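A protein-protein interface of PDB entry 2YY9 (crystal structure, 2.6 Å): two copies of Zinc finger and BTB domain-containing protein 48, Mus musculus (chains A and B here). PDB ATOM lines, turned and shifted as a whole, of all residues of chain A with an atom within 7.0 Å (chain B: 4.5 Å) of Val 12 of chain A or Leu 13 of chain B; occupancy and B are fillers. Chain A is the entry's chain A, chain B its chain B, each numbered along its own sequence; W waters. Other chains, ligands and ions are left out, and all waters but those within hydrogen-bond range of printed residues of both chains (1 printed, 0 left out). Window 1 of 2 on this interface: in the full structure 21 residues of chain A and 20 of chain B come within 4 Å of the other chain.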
ATOM      1  N   GLY A   7      -5.604 -19.115 -13.604  1.00  0.00           N
ATOM      2  CA  GLY A   7      -6.645 -18.868 -14.645  1.00  0.00           C
ATOM      3  C   GLY A   7      -7.681 -17.831 -14.242  1.00  0.00           C
ATOM      4  O   GLY A   7      -8.810 -17.833 -14.746  1.00  0.00           O
ATOM      5  N   HIS A   8      -7.307 -16.942 -13.328  1.00  0.00           N
ATOM      6  CA  HIS A   8      -8.226 -15.908 -12.887  1.00  0.00           C
ATOM      7  C   HIS A   8      -8.734 -15.061 -14.053  1.00  0.00           C
ATOM      8  O   HIS A   8      -9.932 -14.854 -14.200  1.00  0.00           O
ATOM      9  CB  HIS A   8      -7.555 -14.982 -11.880  1.00  0.00           C
ATOM     10  CG  HIS A   8      -8.417 -13.833 -11.472  1.00  0.00           C
ATOM     11  ND1 HIS A   8      -9.403 -13.945 -10.519  1.00  0.00           N
ATOM     12  CD2 HIS A   8      -8.472 -12.556 -11.920  1.00  0.00           C
ATOM     13  CE1 HIS A   8     -10.028 -12.786 -10.394  1.00  0.00           C
ATOM     14  NE2 HIS A   8      -9.482 -11.927 -11.234  1.00  0.00           N
ATOM     15  N   SER A   9      -7.816 -14.572 -14.881  1.00  0.00           N
ATOM     16  CA  SER A   9      -8.202 -13.728 -16.006  1.00  0.00           C
ATOM     17  C   SER A   9      -9.027 -14.465 -17.064  1.00  0.00           C
ATOM     18  O   SER A   9      -9.871 -13.859 -17.718  1.00  0.00           O
ATOM     19  CB  SER A   9      -6.965 -13.084 -16.636  1.00  0.00           C
ATOM     20  OG  SER A   9      -6.197 -14.052 -17.303  1.00  0.00           O
ATOM     21  N   VAL A  10      -8.796 -15.766 -17.224  1.00  0.00           N
ATOM     22  CA  VAL A  10      -9.572 -16.539 -18.187  1.00  0.00           C
ATOM     23  C   VAL A  10     -11.024 -16.561 -17.713  1.00  0.00           C
ATOM     24  O   VAL A  10     -11.939 -16.270 -18.486  1.00  0.00           O
ATOM     25  CB  VAL A  10      -9.066 -17.999 -18.315  1.00  0.00           C
ATOM     26  CG1 VAL A  10     -10.006 -18.801 -19.196  1.00  0.00           C
ATOM     27  CG2 VAL A  10      -7.694 -18.022 -18.928  1.00  0.00           C
ATOM     28  N   ARG A  11     -11.228 -16.895 -16.438  1.00  0.00           N
ATOM     29  CA  ARG A  11     -12.570 -16.943 -15.864  1.00  0.00           C
ATOM     30  C   ARG A  11     -13.290 -15.593 -15.950  1.00  0.00           C
ATOM     31  O   ARG A  11     -14.469 -15.543 -16.301  1.00  0.00           O
ATOM     32  CB  ARG A  11     -12.526 -17.420 -14.402  1.00  0.00           C
ATOM     33  CG  ARG A  11     -12.285 -18.923 -14.252  1.00  0.00           C
ATOM     34  CD  ARG A  11     -12.471 -19.421 -12.813  1.00  0.00           C
ATOM     35  NE  ARG A  11     -11.471 -18.891 -11.883  1.00  0.00           N
ATOM     36  CZ  ARG A  11     -10.182 -19.215 -11.900  1.00  0.00           C
ATOM     37  NH1 ARG A  11      -9.726 -20.077 -12.796  1.00  0.00           N
ATOM     38  NH2 ARG A  11      -9.341 -18.665 -11.031  1.00  0.00           N
ATOM     39  N   VAL A  12     -12.588 -14.506 -15.645  1.00  0.00           N
ATOM     40  CA  VAL A  12     -13.194 -13.173 -15.693  1.00  0.00           C
ATOM     41  C   VAL A  12     -13.670 -12.806 -17.095  1.00  0.00           C
ATOM     42  O   VAL A  12     -14.781 -12.311 -17.274  1.00  0.00           O
ATOM     43  CB  VAL A  12     -12.206 -12.063 -15.213  1.00  0.00           C
ATOM     44  CG1 VAL A  12     -12.767 -10.671 -15.552  1.00  0.00           C
ATOM     45  CG2 VAL A  12     -11.967 -12.188 -13.703  1.00  0.00           C
ATOM     46  N   LEU A  13     -12.828 -13.042 -18.091  1.00  0.00           N
ATOM     47  CA  LEU A  13     -13.214 -12.710 -19.445  1.00  0.00           C
ATOM     48  C   LEU A  13     -14.380 -13.564 -19.935  1.00  0.00           C
ATOM     49  O   LEU A  13     -15.237 -13.060 -20.655  1.00  0.00           O
ATOM     50  CB  LEU A  13     -12.021 -12.817 -20.405  1.00  0.00           C
ATOM     51  CG  LEU A  13     -12.310 -12.150 -21.761  1.00  0.00           C
ATOM     52  CD1 LEU A  13     -12.790 -10.733 -21.546  1.00  0.00           C
ATOM     53  CD2 LEU A  13     -11.076 -12.147 -22.620  1.00  0.00           C
ATOM     54  N   GLN A  14     -14.444 -14.842 -19.564  1.00  0.00           N
ATOM     55  CA  GLN A  14     -15.586 -15.631 -20.020  1.00  0.00           C
ATOM     56  C   GLN A  14     -16.844 -15.262 -19.248  1.00  0.00           C
ATOM     57  O   GLN A  14     -17.954 -15.504 -19.707  1.00  0.00           O
ATOM     58  CB  GLN A  14     -15.325 -17.146 -19.973  1.00  0.00           C
ATOM     59  CG  GLN A  14     -14.461 -17.658 -18.869  1.00  0.00           C
ATOM     60  CD  GLN A  14     -14.055 -19.112 -19.095  1.00  0.00           C
ATOM     61  OE1 GLN A  14     -13.537 -19.468 -20.159  1.00  0.00           O
ATOM     62  NE2 GLN A  14     -14.284 -19.955 -18.092  1.00  0.00           N
ATOM     63  N   GLU A  15     -16.675 -14.652 -18.082  1.00  0.00           N
ATOM     64  CA  GLU A  15     -17.830 -14.210 -17.317  1.00  0.00           C
ATOM     65  C   GLU A  15     -18.288 -12.901 -17.980  1.00  0.00           C
ATOM     66  O   GLU A  15     -19.474 -12.589 -18.012  1.00  0.00           O
ATOM     67  CB  GLU A  15     -17.455 -13.980 -15.847  1.00  0.00           C
ATOM     68  CG  GLU A  15     -18.631 -13.634 -14.936  1.00  0.00           C
ATOM     69  CD  GLU A  15     -19.819 -14.590 -15.082  1.00  0.00           C
ATOM     70  OE1 GLU A  15     -19.629 -15.828 -14.997  1.00  0.00           O
ATOM     71  OE2 GLU A  15     -20.954 -14.098 -15.273  1.00  0.00           O
ATOM     72  N   LEU A  16     -17.344 -12.141 -18.521  1.00  0.00           N
ATOM     73  CA  LEU A  16     -17.701 -10.901 -19.198  1.00  0.00           C
ATOM     74  C   LEU A  16     -18.400 -11.280 -20.496  1.00  0.00           C
ATOM     75  O   LEU A  16     -19.395 -10.668 -20.878  1.00  0.00           O
ATOM     76  CB  LEU A  16     -16.454 -10.048 -19.493  1.00  0.00           C
ATOM     77  CG  LEU A  16     -15.809  -9.319 -18.302  1.00  0.00           C
ATOM     78  CD1 LEU A  16     -14.492  -8.666 -18.728  1.00  0.00           C
ATOM     79  CD2 LEU A  16     -16.781  -8.279 -17.757  1.00  0.00           C
ATOM     80  N   ASN A  17     -17.882 -12.308 -21.164  1.00  0.00           N
ATOM     81  CA  ASN A  17     -18.468 -12.772 -22.407  1.00  0.00           C
ATOM     82  C   ASN A  17     -19.893 -13.241 -22.142  1.00  0.00           C
ATOM     83  O   ASN A  17     -20.808 -12.919 -22.906  1.00  0.00           O
ATOM     84  CB  ASN A  17     -17.658 -13.921 -22.989  1.00  0.00           C
ATOM     85  CG  ASN A  17     -18.076 -14.255 -24.402  1.00  0.00           C
ATOM     86  OD1 ASN A  17     -17.671 -15.270 -24.954  1.00  0.00           O
ATOM     87  ND2 ASN A  17     -18.883 -13.389 -25.002  1.00  0.00           N
ATOM     88  N   LYS A  18     -20.075 -14.007 -21.065  1.00  0.00           N
ATOM     89  CA  LYS A  18     -21.403 -14.485 -20.683  1.00  0.00           C
ATOM     90  C   LYS A  18     -22.296 -13.281 -20.370  1.00  0.00           C
ATOM     91  O   LYS A  18     -23.476 -13.260 -20.719  1.00  0.00           O
ATOM     92  CB  LYS A  18     -21.302 -15.416 -19.466  1.00  0.00           C
ATOM     93  CG  LYS A  18     -21.143 -16.883 -19.859  1.00  0.00           C
ATOM     94  CD  LYS A  18     -20.299 -17.713 -18.887  1.00  0.00           C
ATOM     95  CE  LYS A  18     -20.990 -17.923 -17.548  1.00  0.00           C
ATOM     96  NZ  LYS A  18     -20.318 -19.000 -16.746  1.00  0.00           N
ATOM     97  N   GLN A  19     -21.716 -12.274 -19.723  1.00  0.00           N
ATOM     98  CA  GLN A  19     -22.440 -11.062 -19.385  1.00  0.00           C
ATOM     99  C   GLN A  19     -23.022 -10.357 -20.611  1.00  0.00           C
ATOM    100  O   GLN A  19     -24.209 -10.030 -20.643  1.00  0.00           O
ATOM    101  CB  GLN A  19     -21.525 -10.085 -18.645  1.00  0.00           C
ATOM    102  CG  GLN A  19     -21.452 -10.265 -17.143  1.00  0.00           C
ATOM    103  CD  GLN A  19     -20.423  -9.341 -16.505  1.00  0.00           C
ATOM    104  OE1 GLN A  19     -20.067  -8.308 -17.066  1.00  0.00           O
ATOM    105  NE2 GLN A  19     -19.955  -9.705 -15.322  1.00  0.00           N
ATOM    106  N   CYS A  46     -10.087  -2.146 -25.468  1.00  0.00           N
ATOM    107  CA  CYS A  46      -8.881  -2.967 -25.356  1.00  0.00           C
ATOM    108  C   CYS A  46      -8.353  -3.461 -26.692  1.00  0.00           C
ATOM    109  O   CYS A  46      -7.152  -3.676 -26.852  1.00  0.00           O
ATOM    110  CB  CYS A  46      -9.138  -4.199 -24.488  1.00  0.00           C
ATOM    111  SG  CYS A  46      -9.524  -3.866 -22.778  1.00  0.00           S
ATOM    112  N   SER B   9      -6.759 -13.558 -22.758  1.00  0.00           N
ATOM    113  CA  SER B   9      -7.472 -13.109 -21.567  1.00  0.00           C
ATOM    114  C   SER B   9      -6.557 -12.358 -20.609  1.00  0.00           C
ATOM    115  O   SER B   9      -6.978 -11.415 -19.933  1.00  0.00           O
ATOM    116  CB  SER B   9      -8.110 -14.301 -20.860  1.00  0.00           C
ATOM    117  OG  SER B   9      -9.091 -14.904 -21.689  1.00  0.00           O
ATOM    118  N   VAL B  10      -5.301 -12.782 -20.559  1.00  0.00           N
ATOM    119  CA  VAL B  10      -4.318 -12.143 -19.708  1.00  0.00           C
ATOM    120  C   VAL B  10      -4.108 -10.718 -20.206  1.00  0.00           C
ATOM    121  O   VAL B  10      -4.153  -9.769 -19.425  1.00  0.00           O
ATOM    122  CB  VAL B  10      -2.973 -12.905 -19.751  1.00  0.00           C
ATOM    123  CG1 VAL B  10      -1.858 -12.062 -19.138  1.00  0.00           C
ATOM    124  CG2 VAL B  10      -3.107 -14.232 -19.011  1.00  0.00           C
ATOM    125  N   ARG B  11      -3.891 -10.569 -21.510  1.00  0.00           N
ATOM    126  CA  ARG B  11      -3.664  -9.247 -22.078  1.00  0.00           C
ATOM    127  C   ARG B  11      -4.866  -8.318 -21.928  1.00  0.00           C
ATOM    128  O   ARG B  11      -4.702  -7.143 -21.609  1.00  0.00           O
ATOM    129  CB  ARG B  11      -3.243  -9.362 -23.551  1.00  0.00           C
ATOM    130  CG  ARG B  11      -1.937 -10.147 -23.744  1.00  0.00           C
ATOM    131  CD  ARG B  11      -1.406 -10.098 -25.185  1.00  0.00           C
ATOM    132  NE  ARG B  11      -2.271 -10.793 -26.137  1.00  0.00           N
ATOM    133  CZ  ARG B  11      -2.309 -12.116 -26.294  1.00  0.00           C
ATOM    134  NH1 ARG B  11      -1.520 -12.899 -25.562  1.00  0.00           N
ATOM    135  NH2 ARG B  11      -3.145 -12.655 -27.179  1.00  0.00           N
ATOM    136  N   VAL B  12      -6.075  -8.834 -22.128  1.00  0.00           N
ATOM    137  CA  VAL B  12      -7.257  -7.991 -22.004  1.00  0.00           C
ATOM    138  C   VAL B  12      -7.468  -7.493 -20.572  1.00  0.00           C
ATOM    139  O   VAL B  12      -7.782  -6.323 -20.347  1.00  0.00           O
ATOM    140  CB  VAL B  12      -8.534  -8.729 -22.480  1.00  0.00           C
ATOM    141  CG1 VAL B  12      -9.775  -7.903 -22.134  1.00  0.00           C
ATOM    142  CG2 VAL B  12      -8.471  -8.962 -23.987  1.00  0.00           C
ATOM    143  N   LEU B  13      -7.286  -8.377 -19.601  1.00  0.00           N
ATOM    144  CA  LEU B  13      -7.479  -7.994 -18.211  1.00  0.00           C
ATOM    145  C   LEU B  13      -6.401  -7.019 -17.736  1.00  0.00           C
ATOM    146  O   LEU B  13      -6.651  -6.196 -16.856  1.00  0.00           O
ATOM    147  CB  LEU B  13      -7.504  -9.235 -17.317  1.00  0.00           C
ATOM    148  CG  LEU B  13      -7.983  -8.968 -15.888  1.00  0.00           C
ATOM    149  CD1 LEU B  13      -9.447  -8.509 -15.900  1.00  0.00           C
ATOM    150  CD2 LEU B  13      -7.828 -10.229 -15.047  1.00  0.00           C
ATOM    151  N   GLN B  14      -5.206  -7.106 -18.317  1.00  0.00           N
ATOM    152  CA  GLN B  14      -4.131  -6.205 -17.935  1.00  0.00           C
ATOM    153  C   GLN B  14      -4.412  -4.822 -18.498  1.00  0.00           C
ATOM    154  O   GLN B  14      -3.993  -3.814 -17.930  1.00  0.00           O
ATOM    155  CB  GLN B  14      -2.779  -6.692 -18.460  1.00  0.00           C
ATOM    156  CG  GLN B  14      -2.371  -8.079 -17.991  1.00  0.00           C
ATOM    157  CD  GLN B  14      -0.904  -8.387 -18.268  1.00  0.00           C
ATOM    158  OE1 GLN B  14      -0.044  -8.182 -17.406  1.00  0.00           O
ATOM    159  NE2 GLN B  14      -0.610  -8.870 -19.480  1.00  0.00           N
ATOM    160  N   GLU B  15      -5.120  -4.779 -19.621  1.00  0.00           N
ATOM    161  CA  GLU B  15      -5.460  -3.514 -20.255  1.00  0.00           C
ATOM    162  C   GLU B  15      -6.589  -2.850 -19.474  1.00  0.00           C
ATOM    163  O   GLU B  15      -6.599  -1.636 -19.296  1.00  0.00           O
ATOM    164  CB  GLU B  15      -5.870  -3.751 -21.709  1.00  0.00           C
ATOM    165  CG  GLU B  15      -6.008  -2.482 -22.538  1.00  0.00           C
ATOM    166  CD  GLU B  15      -4.775  -1.581 -22.465  1.00  0.00           C
ATOM    167  OE1 GLU B  15      -3.634  -2.086 -22.639  1.00  0.00           O
ATOM    168  OE2 GLU B  15      -4.954  -0.361 -22.240  1.00  0.00           O
ATOM    169  N   LEU B  16      -7.540  -3.655 -19.010  1.00  0.00           N
ATOM    170  CA  LEU B  16      -8.648  -3.138 -18.218  1.00  0.00           C
ATOM    171  C   LEU B  16      -8.045  -2.662 -16.899  1.00  0.00           C
ATOM    172  O   LEU B  16      -8.482  -1.667 -16.339  1.00  0.00           O
ATOM    173  CB  LEU B  16      -9.693  -4.231 -17.953  1.00  0.00           C
ATOM    174  CG  LEU B  16     -10.532  -4.740 -19.136  1.00  0.00           C
ATOM    175  CD1 LEU B  16     -11.341  -5.971 -18.705  1.00  0.00           C
ATOM    176  CD2 LEU B  16     -11.461  -3.639 -19.638  1.00  0.00           C
ATOM    177  N   ASN B  17      -7.037  -3.375 -16.406  1.00  0.00           N
ATOM    178  CA  ASN B  17      -6.395  -2.981 -15.162  1.00  0.00           C
ATOM    179  C   ASN B  17      -5.753  -1.622 -15.388  1.00  0.00           C
ATOM    180  O   ASN B  17      -5.936  -0.703 -14.602  1.00  0.00           O
ATOM    181  CB  ASN B  17      -5.323  -3.988 -14.745  1.00  0.00           C
ATOM    182  CG  ASN B  17      -4.817  -3.743 -13.329  1.00  0.00           C
ATOM    183  OD1 ASN B  17      -3.943  -4.449 -12.835  1.00  0.00           O
ATOM    184  ND2 ASN B  17      -5.376  -2.740 -12.667  1.00  0.00           N
ATOM    185  N   CYS B  46     -18.112  -9.814 -11.532  1.00  0.00           N
ATOM    186  CA  CYS B  46     -17.529 -11.151 -11.664  1.00  0.00           C
ATOM    187  C   CYS B  46     -16.960 -11.703 -10.364  1.00  0.00           C
ATOM    188  O   CYS B  46     -16.955 -12.909 -10.150  1.00  0.00           O
ATOM    189  CB  CYS B  46     -16.384 -11.149 -12.674  1.00  0.00           C
ATOM    190  SG  CYS B  46     -16.866 -10.730 -14.334  1.00  0.00           S
ATOM    191  N   PHE B  80      -8.874  -8.409  -8.137  1.00  0.00           N
ATOM    192  CA  PHE B  80      -9.933  -8.458  -9.146  1.00  0.00           C
ATOM    193  C   PHE B  80      -9.350  -8.385 -10.555  1.00  0.00           C
ATOM    194  O   PHE B  80      -9.689  -9.184 -11.429  1.00  0.00           O
ATOM    195  CB  PHE B  80     -10.912  -7.289  -8.971  1.00  0.00           C
ATOM    196  CG  PHE B  80     -11.900  -7.470  -7.857  1.00  0.00           C
ATOM    197  CD1 PHE B  80     -11.620  -8.296  -6.773  1.00  0.00           C
ATOM    198  CD2 PHE B  80     -13.099  -6.761  -7.866  1.00  0.00           C
ATOM    199  CE1 PHE B  80     -12.515  -8.411  -5.713  1.00  0.00           C
ATOM    200  CE2 PHE B  80     -14.002  -6.868  -6.810  1.00  0.00           C
ATOM    201  CZ  PHE B  80     -13.708  -7.695  -5.730  1.00  0.00           C
ATOM    202  N   TYR B  81      -8.463  -7.425 -10.765  1.00  0.00           N
ATOM    203  CA  TYR B  81      -7.864  -7.237 -12.072  1.00  0.00           C
ATOM    204  C   TYR B  81      -6.588  -8.018 -12.384  1.00  0.00           C
ATOM    205  O   TYR B  81      -6.101  -7.965 -13.512  1.00  0.00           O
ATOM    206  CB  TYR B  81      -7.618  -5.743 -12.307  1.00  0.00           C
ATOM    207  CG  TYR B  81      -8.889  -4.940 -12.498  1.00  0.00           C
ATOM    208  CD1 TYR B  81      -9.639  -4.504 -11.407  1.00  0.00           C
ATOM    209  CD2 TYR B  81      -9.346  -4.624 -13.779  1.00  0.00           C
ATOM    210  CE1 TYR B  81     -10.814  -3.773 -11.591  1.00  0.00           C
ATOM    211  CE2 TYR B  81     -10.513  -3.899 -13.974  1.00  0.00           C
ATOM    212  CZ  TYR B  81     -11.242  -3.476 -12.880  1.00  0.00           C
ATOM    213  OH  TYR B  81     -12.396  -2.756 -13.080  1.00  0.00           O
ATOM    214  N   THR B  82      -6.042  -8.746 -11.414  1.00  0.00           N
ATOM    215  CA  THR B  82      -4.806  -9.496 -11.666  1.00  0.00           C
ATOM    216  C   THR B  82      -4.839 -10.957 -11.235  1.00  0.00           C
ATOM    217  O   THR B  82      -4.100 -11.775 -11.768  1.00  0.00           O
ATOM    218  CB  THR B  82      -3.603  -8.870 -10.949  1.00  0.00           C
ATOM    219  OG1 THR B  82      -3.712  -9.133  -9.548  1.00  0.00           O
ATOM    220  CG2 THR B  82      -3.552  -7.375 -11.183  1.00  0.00           C
HETATM  221  O   HOH W   1     -11.334 -16.068 -21.484  1.00  0.00           O
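The side-chain sulfur of Cys 46 of chain B lies within hydrogen-bond range of the side-chain amide nitrogen of Gln 19 of chain A, at 3.4 Å. A ring nitrogen (NE2) of His 8 of chain A lies within hydrogen-bond range of the backbone carbonyl oxygen of Phe 80 of chain B, at 2.8 Å.
OE1 of Glu 15 of chain A is in salt-bridge range of NZ of Lys 18 of chain A (3.7 Å).
CD2 of Leu 13 of chain B touches CD2 of His 8 of chain A, at 3.95 Å. O of Ser 9 of chain A touches CB of Ser 9 of chain B, at 3.6 Å. Ser 9 of chain A touches Val 10 of chain B. Ser 9 of chain A touches Leu 13 of chain B (CB to CD2, 3.4 Å). CB of Ser 9 of chain B touches CA of Val 10 of chain A, at 3.8 Å. Ser 9 of chain B touches Leu 13 of chain A (OG to CD2, 3.5 Å). Glu 15 of chain A touches Cys 46 of chain B (CG to SG, 3.5 Å). O of Val 12 of chain B touches SG of Cys 46 of chain A, 3.9 Å away. Cys 46 of chain A touches Glu 15 of chain B (SG to CG, 3.8 Å). Cys 46 of chain A touches Leu 16 of chain B (SG to CD2, 3.7 Å).
Of the printed residues of chain B, His 8 of chain A touches Leu 13 (3.95 Å) and Phe 80 (2.8 Å). Of chain B, only Leu 13 (3.98 Å) and Cys 46 (3.9 Å) come within 4 Å of Val 12 of chain A. Of the printed residues of chain B, Leu 13 of chain A touches Ser 9. Of the printed residues of chain B, Gln 19 of chain A touches Cys 46. Of the printed residues of chain B, Cys 46 of chain A touches Val 12 (3.9 Å), Glu 15 (3.8 Å) and Leu 16 (3.7 Å). Leu 13 of chain B touches three residues of chain A. Of the printed residues of chain A, Leu 16 of chain B touches Cys 46 (3.7 Å). The nearest printed residue of chain B that does not touch Cys 46 of chain A is Arg 11 of chain B (5.9 Å).
Of the 14 printed residues of chain A, 8 touch a printed residue of chain B. Hydrophobic or aromatic side chains of chain A that line the printed part of chain B: His 8, Val 12 and Leu 13. Of the 13 printed residues of chain B, 8 touch a printed residue of chain A. Printed residues of chain B that touch a printed residue of chain A: Ser 9, Val 10, Val 12, Leu 13, Glu 15, Leu 16, Cys 46 and Phe 80. Among the printed residues, 14 pairs touch across the chains. Among the printed residues, no Asp or Glu carboxylate lies within 4 Å of a Lys or Arg side-chain nitrogen of the other chain.
Ser 9 of chain B touches its own counterpart, Ser 9 of chain A. Val 12 of chain A touches Cys 46 of chain B, and with the chains exchanged Cys 46 of chain A touches Val 12 of chain B. Glu 15 of chain A touches Cys 46 of chain B, and with the chains exchanged Cys 46 of chain A touches Glu 15 of chain B. Cys 46 of chain A touches Leu 16 of chain B, but with the chains exchanged Leu 16 of chain A does not touch Cys 46 of chain B (4.2 Å).
Water W1 bridges the side-chain hydroxyl (OG) of Ser 9 of chain B (2.5 Å) and the backbone carbonyl oxygen (O) of Val 10 of chain A (3.1 Å).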
